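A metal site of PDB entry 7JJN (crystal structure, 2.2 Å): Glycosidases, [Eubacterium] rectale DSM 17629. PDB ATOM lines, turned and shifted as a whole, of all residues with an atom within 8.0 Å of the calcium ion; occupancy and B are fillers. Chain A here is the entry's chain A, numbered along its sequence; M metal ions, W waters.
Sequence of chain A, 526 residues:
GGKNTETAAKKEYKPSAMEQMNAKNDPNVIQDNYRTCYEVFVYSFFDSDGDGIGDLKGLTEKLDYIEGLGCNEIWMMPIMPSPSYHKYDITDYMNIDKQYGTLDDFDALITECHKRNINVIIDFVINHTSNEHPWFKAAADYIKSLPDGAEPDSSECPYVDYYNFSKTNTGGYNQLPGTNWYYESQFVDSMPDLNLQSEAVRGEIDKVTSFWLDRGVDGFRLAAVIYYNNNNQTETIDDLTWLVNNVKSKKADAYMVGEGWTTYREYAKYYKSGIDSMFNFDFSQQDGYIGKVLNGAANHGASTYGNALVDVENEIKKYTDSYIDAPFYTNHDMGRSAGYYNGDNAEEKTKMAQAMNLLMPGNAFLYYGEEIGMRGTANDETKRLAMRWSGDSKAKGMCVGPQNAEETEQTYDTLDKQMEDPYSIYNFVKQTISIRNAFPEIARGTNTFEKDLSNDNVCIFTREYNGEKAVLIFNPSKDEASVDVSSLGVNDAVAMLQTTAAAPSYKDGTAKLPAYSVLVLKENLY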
ATOM      1  N   VAL A  42      19.368  10.215  30.698  1.00  0.00           N
ATOM      2  CA  VAL A  42      18.855  10.470  29.363  1.00  0.00           C
ATOM      3  C   VAL A  42      17.847  11.628  29.435  1.00  0.00           C
ATOM      4  O   VAL A  42      17.878  12.520  28.574  1.00  0.00           O
ATOM      5  CB  VAL A  42      18.258   9.198  28.743  1.00  0.00           C
ATOM      6  CG1 VAL A  42      17.410   9.493  27.514  1.00  0.00           C
ATOM      7  CG2 VAL A  42      19.350   8.201  28.389  1.00  0.00           C
ATOM      8  N   TYR A  43      17.007  11.637  30.472  1.00  0.00           N
ATOM      9  CA  TYR A  43      15.971  12.629  30.681  1.00  0.00           C
ATOM     10  C   TYR A  43      16.529  14.061  30.594  1.00  0.00           C
ATOM     11  O   TYR A  43      15.853  14.949  30.071  1.00  0.00           O
ATOM     12  CB  TYR A  43      15.315  12.406  32.048  1.00  0.00           C
ATOM     13  CG  TYR A  43      14.029  13.161  32.324  1.00  0.00           C
ATOM     14  CD1 TYR A  43      14.042  14.427  32.885  1.00  0.00           C
ATOM     15  CD2 TYR A  43      12.796  12.584  32.070  1.00  0.00           C
ATOM     16  CE1 TYR A  43      12.857  15.125  33.131  1.00  0.00           C
ATOM     17  CE2 TYR A  43      11.610  13.245  32.337  1.00  0.00           C
ATOM     18  CZ  TYR A  43      11.643  14.517  32.884  1.00  0.00           C
ATOM     19  OH  TYR A  43      10.464  15.158  33.140  1.00  0.00           O
ATOM     20  N   PHE A  46      20.206  15.444  26.361  1.00  0.00           N
ATOM     21  CA  PHE A  46      20.068  16.145  25.095  1.00  0.00           C
ATOM     22  C   PHE A  46      18.782  15.710  24.388  1.00  0.00           C
ATOM     23  O   PHE A  46      18.530  14.519  24.194  1.00  0.00           O
ATOM     24  CB  PHE A  46      21.306  15.942  24.213  1.00  0.00           C
ATOM     25  CG  PHE A  46      21.398  16.972  23.109  1.00  0.00           C
ATOM     26  CD1 PHE A  46      21.676  18.295  23.396  1.00  0.00           C
ATOM     27  CD2 PHE A  46      21.167  16.621  21.785  1.00  0.00           C
ATOM     28  CE1 PHE A  46      21.744  19.247  22.393  1.00  0.00           C
ATOM     29  CE2 PHE A  46      21.241  17.569  20.776  1.00  0.00           C
ATOM     30  CZ  PHE A  46      21.531  18.874  21.086  1.00  0.00           C
ATOM     31  N   ASP A  47      17.972  16.721  24.044  1.00  0.00           N
ATOM     32  CA  ASP A  47      16.636  16.597  23.459  1.00  0.00           C
ATOM     33  C   ASP A  47      16.746  16.755  21.935  1.00  0.00           C
ATOM     34  O   ASP A  47      17.177  17.784  21.461  1.00  0.00           O
ATOM     35  CB  ASP A  47      15.706  17.657  24.048  1.00  0.00           C
ATOM     36  CG  ASP A  47      14.345  17.793  23.371  1.00  0.00           C
ATOM     37  OD1 ASP A  47      13.833  16.780  22.892  1.00  0.00           O
ATOM     38  OD2 ASP A  47      13.814  18.924  23.339  1.00  0.00           O
ATOM     39  N   SER A  48      16.321  15.733  21.187  1.00  0.00           N
ATOM     40  CA  SER A  48      16.439  15.723  19.728  1.00  0.00           C
ATOM     41  C   SER A  48      15.170  16.252  19.035  1.00  0.00           C
ATOM     42  O   SER A  48      15.261  16.684  17.899  1.00  0.00           O
ATOM     43  CB  SER A  48      16.798  14.348  19.224  1.00  0.00           C
ATOM     44  OG  SER A  48      15.720  13.440  19.411  1.00  0.00           O
ATOM     45  N   ASP A  49      14.001  16.200  19.684  1.00  0.00           N
ATOM     46  CA  ASP A  49      12.730  16.503  18.985  1.00  0.00           C
ATOM     47  C   ASP A  49      12.016  17.750  19.550  1.00  0.00           C
ATOM     48  O   ASP A  49      10.932  18.091  19.097  1.00  0.00           O
ATOM     49  CB  ASP A  49      11.806  15.280  18.958  1.00  0.00           C
ATOM     50  CG  ASP A  49      11.334  14.832  20.330  1.00  0.00           C
ATOM     51  OD1 ASP A  49      11.893  15.291  21.334  1.00  0.00           O
ATOM     52  OD2 ASP A  49      10.400  13.999  20.387  1.00  0.00           O
ATOM     53  N   GLY A  50      12.610  18.434  20.534  1.00  0.00           N
ATOM     54  CA  GLY A  50      12.199  19.781  20.934  1.00  0.00           C
ATOM     55  C   GLY A  50      11.077  19.833  21.972  1.00  0.00           C
ATOM     56  O   GLY A  50      10.472  20.896  22.128  1.00  0.00           O
ATOM     57  N   ASP A  51      10.814  18.733  22.691  1.00  0.00           N
ATOM     58  CA  ASP A  51       9.774  18.679  23.741  1.00  0.00           C
ATOM     59  C   ASP A  51      10.368  19.018  25.117  1.00  0.00           C
ATOM     60  O   ASP A  51       9.659  19.024  26.107  1.00  0.00           O
ATOM     61  CB  ASP A  51       9.072  17.318  23.802  1.00  0.00           C
ATOM     62  CG  ASP A  51       9.969  16.136  24.156  1.00  0.00           C
ATOM     63  OD1 ASP A  51      11.202  16.349  24.379  1.00  0.00           O
ATOM     64  OD2 ASP A  51       9.451  15.008  24.193  1.00  0.00           O
ATOM     65  N   GLY A  52      11.695  19.254  25.172  1.00  0.00           N
ATOM     66  CA  GLY A  52      12.395  19.607  26.414  1.00  0.00           C
ATOM     67  C   GLY A  52      12.831  18.403  27.240  1.00  0.00           C
ATOM     68  O   GLY A  52      13.524  18.551  28.248  1.00  0.00           O
ATOM     69  N   ILE A  53      12.436  17.188  26.823  1.00  0.00           N
ATOM     70  CA  ILE A  53      12.865  15.971  27.505  1.00  0.00           C
ATOM     71  C   ILE A  53      13.974  15.339  26.668  1.00  0.00           C
ATOM     72  O   ILE A  53      13.830  15.214  25.476  1.00  0.00           O
ATOM     73  CB  ILE A  53      11.681  14.997  27.713  1.00  0.00           C
ATOM     74  CG1 ILE A  53      10.450  15.671  28.309  1.00  0.00           C
ATOM     75  CG2 ILE A  53      12.131  13.795  28.538  1.00  0.00           C
ATOM     76  CD1 ILE A  53      10.652  16.201  29.715  1.00  0.00           C
ATOM     77  N   GLY A  54      15.080  14.971  27.307  1.00  0.00           N
ATOM     78  CA  GLY A  54      16.185  14.277  26.650  1.00  0.00           C
ATOM     79  C   GLY A  54      15.781  12.865  26.249  1.00  0.00           C
ATOM     80  O   GLY A  54      14.870  12.259  26.850  1.00  0.00           O
ATOM     81  N   ASP A  55      16.461  12.344  25.225  1.00  0.00           N
ATOM     82  CA  ASP A  55      16.048  11.115  24.555  1.00  0.00           C
ATOM     83  C   ASP A  55      17.280  10.398  24.003  1.00  0.00           C
ATOM     84  O   ASP A  55      18.402  10.931  24.050  1.00  0.00           O
ATOM     85  CB  ASP A  55      14.974  11.426  23.504  1.00  0.00           C
ATOM     86  CG  ASP A  55      15.353  12.545  22.545  1.00  0.00           C
ATOM     87  OD1 ASP A  55      16.262  12.344  21.737  1.00  0.00           O
ATOM     88  OD2 ASP A  55      14.730  13.630  22.619  1.00  0.00           O
ATOM     89  N   LEU A  56      17.069   9.182  23.498  1.00  0.00           N
ATOM     90  CA  LEU A  56      18.148   8.341  22.954  1.00  0.00           C
ATOM     91  C   LEU A  56      18.773   8.976  21.698  1.00  0.00           C
ATOM     92  O   LEU A  56      19.986   8.913  21.506  1.00  0.00           O
ATOM     93  CB  LEU A  56      17.609   6.946  22.634  1.00  0.00           C
ATOM     94  CG  LEU A  56      17.129   6.127  23.825  1.00  0.00           C
ATOM     95  CD1 LEU A  56      16.567   4.794  23.347  1.00  0.00           C
ATOM     96  CD2 LEU A  56      18.247   5.909  24.836  1.00  0.00           C
ATOM     97  N   LYS A  57      17.926   9.542  20.832  1.00  0.00           N
ATOM     98  CA  LYS A  57      18.396  10.188  19.609  1.00  0.00           C
ATOM     99  C   LYS A  57      19.337  11.322  20.001  1.00  0.00           C
ATOM    100  O   LYS A  57      20.379  11.492  19.396  1.00  0.00           O
ATOM    101  CB  LYS A  57      17.221  10.671  18.759  1.00  0.00           C
ATOM    102  CG  LYS A  57      17.475  10.687  17.254  1.00  0.00           C
ATOM    103  CD  LYS A  57      17.573   9.300  16.633  1.00  0.00           C
ATOM    104  CE  LYS A  57      18.797   9.104  15.763  1.00  0.00           C
ATOM    105  NZ  LYS A  57      18.613   8.026  14.751  1.00  0.00           N
ATOM    106  N   GLY A  58      18.963  12.058  21.048  1.00  0.00           N
ATOM    107  CA  GLY A  58      19.745  13.158  21.592  1.00  0.00           C
ATOM    108  C   GLY A  58      21.108  12.694  22.090  1.00  0.00           C
ATOM    109  O   GLY A  58      22.120  13.295  21.764  1.00  0.00           O
ATOM    110  N   LYS A  98       8.563   5.760  26.211  1.00  0.00           N
ATOM    111  CA  LYS A  98       8.175   6.572  25.037  1.00  0.00           C
ATOM    112  C   LYS A  98       8.829   7.960  25.084  1.00  0.00           C
ATOM    113  O   LYS A  98       9.089   8.537  24.043  1.00  0.00           O
ATOM    114  CB  LYS A  98       6.641   6.631  24.894  1.00  0.00           C
ATOM    115  CG  LYS A  98       5.867   7.258  26.053  1.00  0.00           C
ATOM    116  CD  LYS A  98       4.406   7.567  25.721  1.00  0.00           C
ATOM    117  CE  LYS A  98       4.246   8.774  24.809  1.00  0.00           C
ATOM    118  NZ  LYS A  98       2.852   8.948  24.330  1.00  0.00           N
ATOM    119  N   GLN A  99       9.108   8.500  26.278  1.00  0.00           N
ATOM    120  CA  GLN A  99       9.802   9.796  26.426  1.00  0.00           C
ATOM    121  C   GLN A  99      11.230   9.745  25.852  1.00  0.00           C
ATOM    122  O   GLN A  99      11.772  10.784  25.494  1.00  0.00           O
ATOM    123  CB  GLN A  99       9.861  10.242  27.888  1.00  0.00           C
ATOM    124  CG  GLN A  99       8.512  10.643  28.493  1.00  0.00           C
ATOM    125  CD  GLN A  99       8.673  11.273  29.855  1.00  0.00           C
ATOM    126  OE1 GLN A  99       9.322  10.714  30.740  1.00  0.00           O
ATOM    127  NE2 GLN A  99       8.089  12.445  30.029  1.00  0.00           N
ATOM    128  N   TYR A 100      11.830   8.550  25.806  1.00  0.00           N
ATOM    129  CA  TYR A 100      13.220   8.369  25.367  1.00  0.00           C
ATOM    130  C   TYR A 100      13.313   7.961  23.887  1.00  0.00           C
ATOM    131  O   TYR A 100      14.388   8.094  23.294  1.00  0.00           O
ATOM    132  CB  TYR A 100      13.938   7.357  26.256  1.00  0.00           C
ATOM    133  CG  TYR A 100      14.229   7.845  27.656  1.00  0.00           C
ATOM    134  CD1 TYR A 100      14.073   9.174  28.026  1.00  0.00           C
ATOM    135  CD2 TYR A 100      14.680   6.965  28.620  1.00  0.00           C
ATOM    136  CE1 TYR A 100      14.350   9.609  29.316  1.00  0.00           C
ATOM    137  CE2 TYR A 100      14.987   7.378  29.908  1.00  0.00           C
ATOM    138  CZ  TYR A 100      14.822   8.709  30.267  1.00  0.00           C
ATOM    139  OH  TYR A 100      15.121   9.116  31.534  1.00  0.00           O
ATOM    140  N   GLY A 101      12.209   7.482  23.311  1.00  0.00           N
ATOM    141  CA  GLY A 101      12.160   7.025  21.931  1.00  0.00           C
ATOM    142  C   GLY A 101      11.697   5.591  21.834  1.00  0.00           C
ATOM    143  O   GLY A 101      10.833   5.149  22.610  1.00  0.00           O
ATOM    144  N   GLY A 397      18.156  21.645  21.774  1.00  0.00           N
ATOM    145  CA  GLY A 397      18.333  20.379  22.467  1.00  0.00           C
ATOM    146  C   GLY A 397      18.508  20.527  23.969  1.00  0.00           C
ATOM    147  O   GLY A 397      18.642  19.516  24.665  1.00  0.00           O
ATOM    148  N   MET A 398      18.487  21.769  24.460  1.00  0.00           N
ATOM    149  CA  MET A 398      18.553  22.004  25.885  1.00  0.00           C
ATOM    150  C   MET A 398      17.306  21.369  26.521  1.00  0.00           C
ATOM    151  O   MET A 398      16.210  21.467  25.966  1.00  0.00           O
ATOM    152  CB  MET A 398      18.590  23.503  26.199  1.00  0.00           C
ATOM    153  CG  MET A 398      19.181  23.796  27.568  1.00  0.00           C
ATOM    154  SD  MET A 398      20.978  23.568  27.639  1.00  0.00           S
ATOM    155  CE  MET A 398      21.481  24.418  26.146  1.00  0.00           C
ATOM    156  N   CYS A 399      17.512  20.723  27.666  1.00  0.00           N
ATOM    157  CA  CYS A 399      16.475  20.020  28.415  1.00  0.00           C
ATOM    158  C   CYS A 399      15.971  20.942  29.542  1.00  0.00           C
ATOM    159  O   CYS A 399      16.704  21.799  30.022  1.00  0.00           O
ATOM    160  CB  CYS A 399      17.019  18.710  28.959  1.00  0.00           C
ATOM    161  SG  CYS A 399      17.376  17.477  27.672  1.00  0.00           S
HETATM  162 CA    CA M   1      12.800  14.807  23.503  1.00  0.00          CA
HETATM  163  O   HOH W   1      11.705  13.138  24.452  1.00  0.00           O
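Water W1 bridges O of Gln 99 and OD2 of Asp 51.
The calcium ion is bound by water W1. The calcium ion is bound by O of Ile 53, 2.3 Å away. The calcium ion is bound by OD1 of Asp 47, at 2.3 Å. The side-chain carboxylate (OD1) of Asp 51 is bound to the calcium ion (2.4 Å). The calcium ion is bound by OD1 of Asp 49 (2.4 Å). OD2 of Asp 55 binds the calcium ion (2.4 Å).
The side-chain carboxylate (OD2) of Asp 47 sits close to the backbone NH (N) of Gly 50 (3.1 Å). The side-chain carboxylate (OD2) of Asp 47 lies within hydrogen-bond range of the backbone NH (N) of Gly 52 (2.8 Å). SG of Cys 399 sits at hydrogen-bond distance from N of Asp 47 (3.8 Å). The backbone NH (N) of Asp 47 sits at hydrogen-bond distance from the backbone carbonyl oxygen (O) of Gly 397. The side-chain hydroxyl of Ser 48 lies within hydrogen-bond range of the side-chain carboxylate of Asp 55 (2.6 Å). N of Asp 55 is in hydrogen-bond range of O of Phe 46 (3.2 Å). N of Gly 58 lies within hydrogen-bond range of OD1 of Asp 55 (2.8 Å). OD1 of Asp 55 sits close to N of Lys 57 (3.4 Å).
Five residues have an atom within 4 Å of the calcium ion: Asp 47, Asp 49, Asp 51, Ile 53 and Asp 55. Along chain A the residues within 4 Å of the calcium ion span positions 47 to 55. The nearest printed residue that does not touch the calcium ion is Ser 48 (4.3 Å).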
